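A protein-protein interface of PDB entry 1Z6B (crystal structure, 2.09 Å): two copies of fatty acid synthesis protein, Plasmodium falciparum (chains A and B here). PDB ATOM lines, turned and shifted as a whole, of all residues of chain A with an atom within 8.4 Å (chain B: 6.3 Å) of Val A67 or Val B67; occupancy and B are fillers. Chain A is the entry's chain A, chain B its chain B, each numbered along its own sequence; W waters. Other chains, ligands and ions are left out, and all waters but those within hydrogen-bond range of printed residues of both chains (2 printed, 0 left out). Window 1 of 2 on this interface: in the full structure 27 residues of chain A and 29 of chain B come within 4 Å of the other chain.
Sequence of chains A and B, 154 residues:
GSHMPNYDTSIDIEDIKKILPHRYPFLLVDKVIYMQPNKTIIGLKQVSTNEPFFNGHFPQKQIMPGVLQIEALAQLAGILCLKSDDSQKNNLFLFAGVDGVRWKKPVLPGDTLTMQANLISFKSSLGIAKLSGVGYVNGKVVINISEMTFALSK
Water W1 lies within hydrogen-bond range of OE1 of Glu B71 (2.7 Å), N of Gly A66 (3.2 Å) and N of Val A67 (3.2 Å). Water W2 lies within hydrogen-bond range of the side-chain carboxylate (OE1) of Glu A71 (2.7 Å), the backbone NH (N) of Val B67 (3.1 Å) and the backbone NH (N) of Gly B66 (3.2 Å).
Pro B65 touches Phe A26 (CG to CE2, 3.6 Å). CZ of Phe A26 touches CG2 of Val B67, 3.97 Å away. Phe B26 touches Pro A65 (CE2 to CG, 3.6 Å). Phe B26 touches Val A67. Val A67 touches Ile B70. Glu B71 touches Val A67 (OE1 to CG1, 3.7 Å). Glu A71 touches Val B67. Val B67 touches Phe A95 (CG1 to CE2, 3.6 Å). CH2 of Trp B103 touches CG1 of Val A98 (3.9 Å). CE3 of Trp A103 touches O of Phe B95, 3.1 Å away.
O of Gly A66 is in hydrogen-bond range of NE1 of Trp A103 (2.9 Å). The side-chain amide nitrogen of Gln A75 is in hydrogen-bond range of the side-chain carboxylate of Glu A71. The backbone carbonyl oxygen of Phe A26 is in hydrogen-bond range of the side-chain amide nitrogen of Gln A75. The backbone carbonyl oxygen (O) of Gly B66 is in hydrogen-bond range of the indole nitrogen (NE1) of Trp B103 (3.1 Å).
Phe A26 touches Pro B65, and with the chains exchanged Pro A65 touches Phe B26. Phe A26 touches Val B67, and with the chains exchanged Val A67 touches Phe B26. Val A67 touches Ile B70, but with the chains exchanged Ile A70 does not touch Val B67 (4.05 Å). Phe A95 touches Val B67, but with the chains exchanged Val A67 does not touch Phe B95 (4.1 Å). Positions printed for both chains: 26, 64, 65, 66, 67, 68, 69, 70, 71, 72, 74, 95 and 103.
Met A64 touches none of the printed residues of chain B. Printed residues of chain B within 4 Å of Val A67: Phe B26, Val B67, Ile B70 and Glu B71. Leu A68 touches none of the printed residues of chain B. Of the printed residues of chain B, Glu A71 touches Val B67. Of the printed residues of chain B, Phe A95 touches Val B67 and Trp B103. No residue of chain A comes within 4 Å of Gly B66. Printed residues of chain A within 4 Å of Glu B71: Val A67. Of the printed residues of chain A, Phe B95 touches Trp A103. The nearest printed residue of chain B that does not touch Val A67 is Phe B95 (4.1 Å). The nearest printed residue of chain A that does not touch Glu B71 is His A57 (4.3 Å).
Of the 23 printed residues of chain A, 8 touch a printed residue of chain B. Hydrophobic or aromatic side chains of chain B that line the printed part of chain A: Phe B26, Pro B65, Val B67, Ile B70, Phe B95 and Trp B103. Among the printed residues, 13 pairs touch across the chains.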
ATOM      1  N   PHE A  26      21.816  23.814  -1.961  1.00  0.00           N
ATOM      2  CA  PHE A  26      20.710  24.642  -2.389  1.00  0.00           C
ATOM      3  C   PHE A  26      21.102  26.068  -2.766  1.00  0.00           C
ATOM      4  O   PHE A  26      20.282  26.988  -2.648  1.00  0.00           O
ATOM      5  CB  PHE A  26      19.605  24.627  -1.310  1.00  0.00           C
ATOM      6  CG  PHE A  26      18.236  24.462  -1.884  1.00  0.00           C
ATOM      7  CD1 PHE A  26      17.789  23.203  -2.295  1.00  0.00           C
ATOM      8  CD2 PHE A  26      17.412  25.536  -2.046  1.00  0.00           C
ATOM      9  CE1 PHE A  26      16.539  23.039  -2.859  1.00  0.00           C
ATOM     10  CE2 PHE A  26      16.155  25.375  -2.590  1.00  0.00           C
ATOM     11  CZ  PHE A  26      15.724  24.121  -3.011  1.00  0.00           C
ATOM     12  N   LEU A  28      22.115  27.988  -6.126  1.00  0.00           N
ATOM     13  CA  LEU A  28      21.872  27.699  -7.543  1.00  0.00           C
ATOM     14  C   LEU A  28      22.157  28.921  -8.441  1.00  0.00           C
ATOM     15  O   LEU A  28      21.559  29.093  -9.511  1.00  0.00           O
ATOM     16  CB  LEU A  28      20.425  27.212  -7.706  1.00  0.00           C
ATOM     17  CG  LEU A  28      20.132  25.916  -6.931  1.00  0.00           C
ATOM     18  CD1 LEU A  28      18.627  25.628  -6.867  1.00  0.00           C
ATOM     19  CD2 LEU A  28      20.932  24.771  -7.550  1.00  0.00           C
ATOM     20  N   HIS A  57      16.054  12.739 -10.451  1.00  0.00           N
ATOM     21  CA  HIS A  57      15.201  13.447 -11.386  1.00  0.00           C
ATOM     22  C   HIS A  57      15.788  13.494 -12.796  1.00  0.00           C
ATOM     23  O   HIS A  57      16.177  14.570 -13.277  1.00  0.00           O
ATOM     24  CB  HIS A  57      14.910  14.854 -10.806  1.00  0.00           C
ATOM     25  CG  HIS A  57      13.787  15.588 -11.479  1.00  0.00           C
ATOM     26  ND1 HIS A  57      13.923  16.159 -12.729  1.00  0.00           N
ATOM     27  CD2 HIS A  57      12.533  15.884 -11.064  1.00  0.00           C
ATOM     28  CE1 HIS A  57      12.785  16.742 -13.072  1.00  0.00           C
ATOM     29  NE2 HIS A  57      11.929  16.602 -12.074  1.00  0.00           N
ATOM     30  N   MET A  64      16.858  18.983 -15.341  1.00  0.00           N
ATOM     31  CA  MET A  64      16.863  19.835 -14.161  1.00  0.00           C
ATOM     32  C   MET A  64      15.423  20.132 -13.766  1.00  0.00           C
ATOM     33  O   MET A  64      14.661  20.589 -14.605  1.00  0.00           O
ATOM     34  CB  MET A  64      17.612  21.148 -14.432  1.00  0.00           C
ATOM     35  CG  MET A  64      17.723  22.032 -13.206  1.00  0.00           C
ATOM     36  SD  MET A  64      18.575  23.566 -13.620  1.00  0.00           S
ATOM     37  CE  MET A  64      18.383  24.468 -12.078  1.00  0.00           C
ATOM     38  N   PRO A  65      15.035  19.884 -12.510  1.00  0.00           N
ATOM     39  CA  PRO A  65      13.674  20.159 -12.090  1.00  0.00           C
ATOM     40  C   PRO A  65      13.253  21.583 -12.343  1.00  0.00           C
ATOM     41  O   PRO A  65      13.992  22.502 -12.009  1.00  0.00           O
ATOM     42  CB  PRO A  65      13.705  19.868 -10.555  1.00  0.00           C
ATOM     43  CG  PRO A  65      14.781  18.959 -10.343  1.00  0.00           C
ATOM     44  CD  PRO A  65      15.821  19.297 -11.410  1.00  0.00           C
ATOM     45  N   GLY A  66      12.056  21.766 -12.878  1.00  0.00           N
ATOM     46  CA  GLY A  66      11.505  23.097 -13.101  1.00  0.00           C
ATOM     47  C   GLY A  66      11.434  23.975 -11.855  1.00  0.00           C
ATOM     48  O   GLY A  66      11.597  25.200 -11.934  1.00  0.00           O
ATOM     49  N   VAL A  67      11.156  23.378 -10.704  1.00  0.00           N
ATOM     50  CA  VAL A  67      11.094  24.145  -9.452  1.00  0.00           C
ATOM     51  C   VAL A  67      12.484  24.657  -9.021  1.00  0.00           C
ATOM     52  O   VAL A  67      12.573  25.642  -8.274  1.00  0.00           O
ATOM     53  CB  VAL A  67      10.467  23.359  -8.242  1.00  0.00           C
ATOM     54  CG1 VAL A  67       9.006  23.005  -8.494  1.00  0.00           C
ATOM     55  CG2 VAL A  67      11.243  22.149  -7.912  1.00  0.00           C
ATOM     56  N   LEU A  68      13.554  23.977  -9.438  1.00  0.00           N
ATOM     57  CA  LEU A  68      14.924  24.475  -9.142  1.00  0.00           C
ATOM     58  C   LEU A  68      15.325  25.615 -10.069  1.00  0.00           C
ATOM     59  O   LEU A  68      16.169  26.419  -9.688  1.00  0.00           O
ATOM     60  CB  LEU A  68      15.983  23.367  -9.143  1.00  0.00           C
ATOM     61  CG  LEU A  68      15.823  22.362  -7.987  1.00  0.00           C
ATOM     62  CD1 LEU A  68      16.997  21.444  -7.923  1.00  0.00           C
ATOM     63  CD2 LEU A  68      15.620  23.027  -6.619  1.00  0.00           C
ATOM     64  N   GLN A  69      14.721  25.669 -11.269  1.00  0.00           N
ATOM     65  CA  GLN A  69      14.872  26.787 -12.182  1.00  0.00           C
ATOM     66  C   GLN A  69      14.169  28.033 -11.625  1.00  0.00           C
ATOM     67  O   GLN A  69      14.652  29.128 -11.788  1.00  0.00           O
ATOM     68  CB  GLN A  69      14.339  26.447 -13.569  1.00  0.00           C
ATOM     69  CG  GLN A  69      14.889  25.180 -14.158  1.00  0.00           C
ATOM     70  CD  GLN A  69      14.281  24.853 -15.487  1.00  0.00           C
ATOM     71  OE1 GLN A  69      13.830  25.743 -16.211  1.00  0.00           O
ATOM     72  NE2 GLN A  69      14.255  23.569 -15.820  1.00  0.00           N
ATOM     73  N   ILE A  70      13.033  27.852 -10.961  1.00  0.00           N
ATOM     74  CA  ILE A  70      12.396  28.929 -10.197  1.00  0.00           C
ATOM     75  C   ILE A  70      13.338  29.338  -9.055  1.00  0.00           C
ATOM     76  O   ILE A  70      13.477  30.512  -8.750  1.00  0.00           O
ATOM     77  CB  ILE A  70      11.038  28.488  -9.543  1.00  0.00           C
ATOM     78  CG1 ILE A  70       9.972  28.124 -10.577  1.00  0.00           C
ATOM     79  CG2 ILE A  70      10.500  29.589  -8.646  1.00  0.00           C
ATOM     80  CD1 ILE A  70       8.741  27.440  -9.960  1.00  0.00           C
ATOM     81  N   GLU A  71      13.934  28.360  -8.386  1.00  0.00           N
ATOM     82  CA  GLU A  71      14.763  28.660  -7.235  1.00  0.00           C
ATOM     83  C   GLU A  71      16.027  29.448  -7.625  1.00  0.00           C
ATOM     84  O   GLU A  71      16.425  30.360  -6.908  1.00  0.00           O
ATOM     85  CB  GLU A  71      15.104  27.378  -6.474  1.00  0.00           C
ATOM     86  CG  GLU A  71      16.040  27.561  -5.274  1.00  0.00           C
ATOM     87  CD  GLU A  71      15.437  28.390  -4.132  1.00  0.00           C
ATOM     88  OE1 GLU A  71      14.193  28.527  -4.069  1.00  0.00           O
ATOM     89  OE2 GLU A  71      16.219  28.892  -3.287  1.00  0.00           O
ATOM     90  N   ALA A  72      16.639  29.110  -8.758  1.00  0.00           N
ATOM     91  CA  ALA A  72      17.831  29.814  -9.223  1.00  0.00           C
ATOM     92  C   ALA A  72      17.503  31.284  -9.634  1.00  0.00           C
ATOM     93  O   ALA A  72      18.248  32.203  -9.329  1.00  0.00           O
ATOM     94  CB  ALA A  72      18.488  29.025 -10.363  1.00  0.00           C
ATOM     95  N   LEU A  73      16.364  31.486 -10.282  1.00  0.00           N
ATOM     96  CA  LEU A  73      15.831  32.815 -10.573  1.00  0.00           C
ATOM     97  C   LEU A  73      15.492  33.612  -9.325  1.00  0.00           C
ATOM     98  O   LEU A  73      15.691  34.833  -9.292  1.00  0.00           O
ATOM     99  CB  LEU A  73      14.612  32.723 -11.498  1.00  0.00           C
ATOM    100  CG  LEU A  73      15.008  32.798 -12.983  1.00  0.00           C
ATOM    101  CD1 LEU A  73      13.832  32.478 -13.861  1.00  0.00           C
ATOM    102  CD2 LEU A  73      15.627  34.148 -13.360  1.00  0.00           C
ATOM    103  N   ALA A  74      14.988  32.928  -8.311  1.00  0.00           N
ATOM    104  CA  ALA A  74      14.650  33.540  -7.025  1.00  0.00           C
ATOM    105  C   ALA A  74      15.879  34.020  -6.291  1.00  0.00           C
ATOM    106  O   ALA A  74      15.872  35.120  -5.691  1.00  0.00           O
ATOM    107  CB  ALA A  74      13.871  32.564  -6.137  1.00  0.00           C
ATOM    108  N   GLN A  75      16.931  33.201  -6.336  1.00  0.00           N
ATOM    109  CA  GLN A  75      18.168  33.501  -5.638  1.00  0.00           C
ATOM    110  C   GLN A  75      18.923  34.687  -6.305  1.00  0.00           C
ATOM    111  O   GLN A  75      19.357  35.618  -5.624  1.00  0.00           O
ATOM    112  CB  GLN A  75      19.033  32.256  -5.563  1.00  0.00           C
ATOM    113  CG  GLN A  75      18.585  31.283  -4.498  1.00  0.00           C
ATOM    114  CD  GLN A  75      19.365  30.004  -4.516  1.00  0.00           C
ATOM    115  OE1 GLN A  75      20.503  29.987  -4.996  1.00  0.00           O
ATOM    116  NE2 GLN A  75      18.794  28.943  -3.917  1.00  0.00           N
ATOM    117  N   PHE A  95      10.266  32.796  -0.106  1.00  0.00           N
ATOM    118  CA  PHE A  95       9.233  32.821  -1.140  1.00  0.00           C
ATOM    119  C   PHE A  95       7.850  33.038  -0.495  1.00  0.00           C
ATOM    120  O   PHE A  95       7.434  32.247   0.356  1.00  0.00           O
ATOM    121  CB  PHE A  95       9.245  31.513  -1.938  1.00  0.00           C
ATOM    122  CG  PHE A  95       9.585  31.689  -3.383  1.00  0.00           C
ATOM    123  CD1 PHE A  95       8.941  32.638  -4.144  1.00  0.00           C
ATOM    124  CD2 PHE A  95      10.510  30.872  -3.991  1.00  0.00           C
ATOM    125  CE1 PHE A  95       9.257  32.797  -5.478  1.00  0.00           C
ATOM    126  CE2 PHE A  95      10.822  31.021  -5.329  1.00  0.00           C
ATOM    127  CZ  PHE A  95      10.190  31.979  -6.075  1.00  0.00           C
ATOM    128  N   VAL A  98       4.397  33.123  -6.118  1.00  0.00           N
ATOM    129  CA  VAL A  98       4.907  33.093  -7.492  1.00  0.00           C
ATOM    130  C   VAL A  98       3.722  32.884  -8.441  1.00  0.00           C
ATOM    131  O   VAL A  98       2.835  32.060  -8.179  1.00  0.00           O
ATOM    132  CB  VAL A  98       6.042  32.010  -7.673  1.00  0.00           C
ATOM    133  CG1 VAL A  98       5.498  30.587  -7.605  1.00  0.00           C
ATOM    134  CG2 VAL A  98       6.823  32.214  -8.971  1.00  0.00           C
ATOM    135  N   VAL A 101       4.357  30.992 -13.923  1.00  0.00           N
ATOM    136  CA  VAL A 101       5.530  30.243 -14.325  1.00  0.00           C
ATOM    137  C   VAL A 101       5.151  29.357 -15.511  1.00  0.00           C
ATOM    138  O   VAL A 101       4.204  28.569 -15.433  1.00  0.00           O
ATOM    139  CB  VAL A 101       6.056  29.364 -13.211  1.00  0.00           C
ATOM    140  CG1 VAL A 101       7.345  28.683 -13.646  1.00  0.00           C
ATOM    141  CG2 VAL A 101       6.243  30.168 -11.928  1.00  0.00           C
ATOM    142  N   TRP A 103       7.256  26.743 -18.122  1.00  0.00           N
ATOM    143  CA  TRP A 103       8.466  26.061 -18.509  1.00  0.00           C
ATOM    144  C   TRP A 103       8.363  25.718 -19.990  1.00  0.00           C
ATOM    145  O   TRP A 103       7.422  25.050 -20.402  1.00  0.00           O
ATOM    146  CB  TRP A 103       8.623  24.806 -17.676  1.00  0.00           C
ATOM    147  CG  TRP A 103       8.967  25.066 -16.259  1.00  0.00           C
ATOM    148  CD1 TRP A 103      10.171  25.449 -15.785  1.00  0.00           C
ATOM    149  CD2 TRP A 103       8.119  24.915 -15.108  1.00  0.00           C
ATOM    150  NE1 TRP A 103      10.129  25.578 -14.420  1.00  0.00           N
ATOM    151  CE2 TRP A 103       8.877  25.249 -13.980  1.00  0.00           C
ATOM    152  CE3 TRP A 103       6.793  24.532 -14.920  1.00  0.00           C
ATOM    153  CZ2 TRP A 103       8.361  25.196 -12.685  1.00  0.00           C
ATOM    154  CZ3 TRP A 103       6.280  24.507 -13.637  1.00  0.00           C
ATOM    155  CH2 TRP A 103       7.061  24.837 -12.539  1.00  0.00           C
ATOM    156  N   ILE A 143      12.387  29.209 -19.397  1.00  0.00           N
ATOM    157  CA  ILE A 143      11.450  29.494 -18.317  1.00  0.00           C
ATOM    158  C   ILE A 143      11.084  30.988 -18.295  1.00  0.00           C
ATOM    159  O   ILE A 143      11.941  31.843 -18.500  1.00  0.00           O
ATOM    160  CB  ILE A 143      12.017  29.002 -16.940  1.00  0.00           C
ATOM    161  CG1 ILE A 143      10.986  29.168 -15.813  1.00  0.00           C
ATOM    162  CG2 ILE A 143      13.316  29.723 -16.587  1.00  0.00           C
ATOM    163  CD1 ILE A 143      11.489  28.790 -14.480  1.00  0.00           C
ATOM    164  N   ILE A 145       8.793  33.650 -15.603  1.00  0.00           N
ATOM    165  CA  ILE A 145       8.077  33.849 -14.339  1.00  0.00           C
ATOM    166  C   ILE A 145       7.533  35.265 -14.319  1.00  0.00           C
ATOM    167  O   ILE A 145       8.307  36.212 -14.318  1.00  0.00           O
ATOM    168  CB  ILE A 145       9.022  33.633 -13.120  1.00  0.00           C
ATOM    169  CG1 ILE A 145       9.632  32.233 -13.164  1.00  0.00           C
ATOM    170  CG2 ILE A 145       8.257  33.893 -11.812  1.00  0.00           C
ATOM    171  CD1 ILE A 145      10.719  31.989 -12.151  1.00  0.00           C
ATOM    172  N   MET A 148       7.621  36.916  -9.046  1.00  0.00           N
ATOM    173  CA  MET A 148       8.058  36.267  -7.818  1.00  0.00           C
ATOM    174  C   MET A 148       7.952  37.287  -6.714  1.00  0.00           C
ATOM    175  O   MET A 148       8.460  38.399  -6.855  1.00  0.00           O
ATOM    176  CB  MET A 148       9.520  35.851  -7.910  1.00  0.00           C
ATOM    177  CG  MET A 148       9.863  34.960  -9.057  1.00  0.00           C
ATOM    178  SD  MET A 148      11.638  34.732  -9.102  1.00  0.00           S
ATOM    179  CE  MET A 148      12.145  36.126 -10.101  1.00  0.00           C
ATOM    180  N   PHE A 150       8.712  37.994  -2.599  1.00  0.00           N
ATOM    181  CA  PHE A 150       9.537  37.584  -1.474  1.00  0.00           C
ATOM    182  C   PHE A 150       9.224  38.454  -0.277  1.00  0.00           C
ATOM    183  O   PHE A 150       9.138  39.674  -0.392  1.00  0.00           O
ATOM    184  CB  PHE A 150      11.037  37.714  -1.824  1.00  0.00           C
ATOM    185  CG  PHE A 150      11.411  36.998  -3.078  1.00  0.00           C
ATOM    186  CD1 PHE A 150      11.463  35.627  -3.101  1.00  0.00           C
ATOM    187  CD2 PHE A 150      11.661  37.701  -4.247  1.00  0.00           C
ATOM    188  CE1 PHE A 150      11.778  34.962  -4.257  1.00  0.00           C
ATOM    189  CE2 PHE A 150      11.970  37.036  -5.414  1.00  0.00           C
ATOM    190  CZ  PHE A 150      12.021  35.669  -5.421  1.00  0.00           C
ATOM    191  N   PHE B  26      14.984  13.536  -4.669  1.00  0.00           N
ATOM    192  CA  PHE B  26      13.903  14.329  -5.243  1.00  0.00           C
ATOM    193  C   PHE B  26      12.539  13.636  -5.273  1.00  0.00           C
ATOM    194  O   PHE B  26      11.695  14.006  -6.088  1.00  0.00           O
ATOM    195  CB  PHE B  26      14.298  14.853  -6.630  1.00  0.00           C
ATOM    196  CG  PHE B  26      14.047  16.310  -6.785  1.00  0.00           C
ATOM    197  CD1 PHE B  26      14.920  17.235  -6.207  1.00  0.00           C
ATOM    198  CD2 PHE B  26      12.929  16.779  -7.442  1.00  0.00           C
ATOM    199  CE1 PHE B  26      14.664  18.578  -6.280  1.00  0.00           C
ATOM    200  CE2 PHE B  26      12.705  18.143  -7.544  1.00  0.00           C
ATOM    201  CZ  PHE B  26      13.556  19.033  -6.962  1.00  0.00           C
ATOM    202  N   MET B  64      11.954  24.610   5.140  1.00  0.00           N
ATOM    203  CA  MET B  64      11.767  23.837   3.911  1.00  0.00           C
ATOM    204  C   MET B  64      11.555  24.793   2.750  1.00  0.00           C
ATOM    205  O   MET B  64      10.640  25.613   2.792  1.00  0.00           O
ATOM    206  CB  MET B  64      10.571  22.899   4.008  1.00  0.00           C
ATOM    207  CG  MET B  64      10.416  21.976   2.768  1.00  0.00           C
ATOM    208  SD  MET B  64       8.971  20.891   2.855  1.00  0.00           S
ATOM    209  CE  MET B  64       9.126  20.086   1.252  1.00  0.00           C
ATOM    210  N   PRO B  65      12.382  24.720   1.712  1.00  0.00           N
ATOM    211  CA  PRO B  65      12.220  25.647   0.594  1.00  0.00           C
ATOM    212  C   PRO B  65      10.798  25.580   0.080  1.00  0.00           C
ATOM    213  O   PRO B  65      10.277  24.483  -0.112  1.00  0.00           O
ATOM    214  CB  PRO B  65      13.180  25.116  -0.457  1.00  0.00           C
ATOM    215  CG  PRO B  65      14.177  24.388   0.295  1.00  0.00           C
ATOM    216  CD  PRO B  65      13.515  23.818   1.507  1.00  0.00           C
ATOM    217  N   GLY B  66      10.175  26.744  -0.107  1.00  0.00           N
ATOM    218  CA  GLY B  66       8.900  26.826  -0.778  1.00  0.00           C
ATOM    219  C   GLY B  66       8.808  26.050  -2.081  1.00  0.00           C
ATOM    220  O   GLY B  66       7.798  25.418  -2.340  1.00  0.00           O
ATOM    221  N   VAL B  67       9.851  26.102  -2.907  1.00  0.00           N
ATOM    222  CA  VAL B  67       9.788  25.469  -4.217  1.00  0.00           C
ATOM    223  C   VAL B  67       9.666  23.937  -4.109  1.00  0.00           C
ATOM    224  O   VAL B  67       9.127  23.301  -5.017  1.00  0.00           O
ATOM    225  CB  VAL B  67      10.955  25.858  -5.123  1.00  0.00           C
ATOM    226  CG1 VAL B  67      11.017  27.399  -5.283  1.00  0.00           C
ATOM    227  CG2 VAL B  67      12.272  25.237  -4.629  1.00  0.00           C
ATOM    228  N   LEU B  68      10.144  23.371  -2.998  1.00  0.00           N
ATOM    229  CA  LEU B  68      10.045  21.929  -2.762  1.00  0.00           C
ATOM    230  C   LEU B  68       8.663  21.548  -2.265  1.00  0.00           C
ATOM    231  O   LEU B  68       8.264  20.402  -2.383  1.00  0.00           O
ATOM    232  CB  LEU B  68      11.087  21.468  -1.748  1.00  0.00           C
ATOM    233  CG  LEU B  68      12.533  21.536  -2.236  1.00  0.00           C
ATOM    234  CD1 LEU B  68      13.421  20.856  -1.254  1.00  0.00           C
ATOM    235  CD2 LEU B  68      12.710  20.948  -3.627  1.00  0.00           C
ATOM    236  N   GLN B  69       7.936  22.515  -1.704  1.00  0.00           N
ATOM    237  CA  GLN B  69       6.531  22.320  -1.375  1.00  0.00           C
ATOM    238  C   GLN B  69       5.677  22.302  -2.643  1.00  0.00           C
ATOM    239  O   GLN B  69       4.727  21.516  -2.740  1.00  0.00           O
ATOM    240  CB  GLN B  69       6.010  23.370  -0.395  1.00  0.00           C
ATOM    241  CG  GLN B  69       6.876  23.589   0.818  1.00  0.00           C
ATOM    242  CD  GLN B  69       6.351  24.684   1.736  1.00  0.00           C
ATOM    243  OE1 GLN B  69       5.164  24.921   1.795  1.00  0.00           O
ATOM    244  NE2 GLN B  69       7.244  25.304   2.495  1.00  0.00           N
ATOM    245  N   ILE B  70       5.997  23.153  -3.609  1.00  0.00           N
ATOM    246  CA  ILE B  70       5.367  23.054  -4.928  1.00  0.00           C
ATOM    247  C   ILE B  70       5.605  21.647  -5.480  1.00  0.00           C
ATOM    248  O   ILE B  70       4.685  20.980  -5.956  1.00  0.00           O
ATOM    249  CB  ILE B  70       5.928  24.080  -5.898  1.00  0.00           C
ATOM    250  CG1 ILE B  70       5.524  25.526  -5.505  1.00  0.00           C
ATOM    251  CG2 ILE B  70       5.462  23.770  -7.360  1.00  0.00           C
ATOM    252  CD1 ILE B  70       6.215  26.578  -6.375  1.00  0.00           C
ATOM    253  N   GLU B  71       6.853  21.206  -5.415  1.00  0.00           N
ATOM    254  CA  GLU B  71       7.245  19.939  -5.999  1.00  0.00           C
ATOM    255  C   GLU B  71       6.538  18.744  -5.333  1.00  0.00           C
ATOM    256  O   GLU B  71       6.159  17.775  -6.006  1.00  0.00           O
ATOM    257  CB  GLU B  71       8.782  19.810  -5.908  1.00  0.00           C
ATOM    258  CG  GLU B  71       9.350  18.499  -6.409  1.00  0.00           C
ATOM    259  CD  GLU B  71       9.199  18.309  -7.899  1.00  0.00           C
ATOM    260  OE1 GLU B  71       8.956  19.314  -8.628  1.00  0.00           O
ATOM    261  OE2 GLU B  71       9.396  17.148  -8.335  1.00  0.00           O
ATOM    262  N   ALA B  72       6.380  18.789  -4.017  1.00  0.00           N
ATOM    263  CA  ALA B  72       5.721  17.721  -3.312  1.00  0.00           C
ATOM    264  C   ALA B  72       4.252  17.649  -3.804  1.00  0.00           C
ATOM    265  O   ALA B  72       3.770  16.580  -4.172  1.00  0.00           O
ATOM    266  CB  ALA B  72       5.800  17.943  -1.819  1.00  0.00           C
ATOM    267  N   ALA B  74       3.091  18.808  -6.597  1.00  0.00           N
ATOM    268  CA  ALA B  74       3.135  18.448  -8.016  1.00  0.00           C
ATOM    269  C   ALA B  74       3.336  16.933  -8.225  1.00  0.00           C
ATOM    270  O   ALA B  74       2.750  16.326  -9.129  1.00  0.00           O
ATOM    271  CB  ALA B  74       4.251  19.215  -8.697  1.00  0.00           C
ATOM    272  N   PHE B  95       5.952  18.980 -15.726  1.00  0.00           N
ATOM    273  CA  PHE B  95       5.412  20.162 -15.099  1.00  0.00           C
ATOM    274  C   PHE B  95       5.581  21.302 -16.116  1.00  0.00           C
ATOM    275  O   PHE B  95       6.694  21.746 -16.371  1.00  0.00           O
ATOM    276  CB  PHE B  95       6.251  20.446 -13.845  1.00  0.00           C
ATOM    277  CG  PHE B  95       5.522  21.115 -12.706  1.00  0.00           C
ATOM    278  CD1 PHE B  95       4.250  21.648 -12.838  1.00  0.00           C
ATOM    279  CD2 PHE B  95       6.187  21.256 -11.485  1.00  0.00           C
ATOM    280  CE1 PHE B  95       3.654  22.275 -11.776  1.00  0.00           C
ATOM    281  CE2 PHE B  95       5.592  21.869 -10.419  1.00  0.00           C
ATOM    282  CZ  PHE B  95       4.327  22.389 -10.565  1.00  0.00           C
ATOM    283  N   TRP B 103       2.551  30.997  -0.244  1.00  0.00           N
ATOM    284  CA  TRP B 103       3.074  30.353   0.968  1.00  0.00           C
ATOM    285  C   TRP B 103       2.659  31.179   2.162  1.00  0.00           C
ATOM    286  O   TRP B 103       2.844  32.391   2.157  1.00  0.00           O
ATOM    287  CB  TRP B 103       4.596  30.302   0.935  1.00  0.00           C
ATOM    288  CG  TRP B 103       5.148  29.372  -0.071  1.00  0.00           C
ATOM    289  CD1 TRP B 103       5.310  28.052   0.071  1.00  0.00           C
ATOM    290  CD2 TRP B 103       5.572  29.696  -1.394  1.00  0.00           C
ATOM    291  NE1 TRP B 103       5.840  27.510  -1.075  1.00  0.00           N
ATOM    292  CE2 TRP B 103       6.016  28.508  -1.992  1.00  0.00           C
ATOM    293  CE3 TRP B 103       5.631  30.880  -2.136  1.00  0.00           C
ATOM    294  CZ2 TRP B 103       6.518  28.462  -3.289  1.00  0.00           C
ATOM    295  CZ3 TRP B 103       6.132  30.833  -3.421  1.00  0.00           C
ATOM    296  CH2 TRP B 103       6.572  29.634  -3.982  1.00  0.00           C
HETATM  297  O   HOH W   1      10.217  20.322 -10.751  1.00  0.00           O
HETATM  298  O   HOH W   2      12.233  27.960  -2.243  1.00  0.00           O
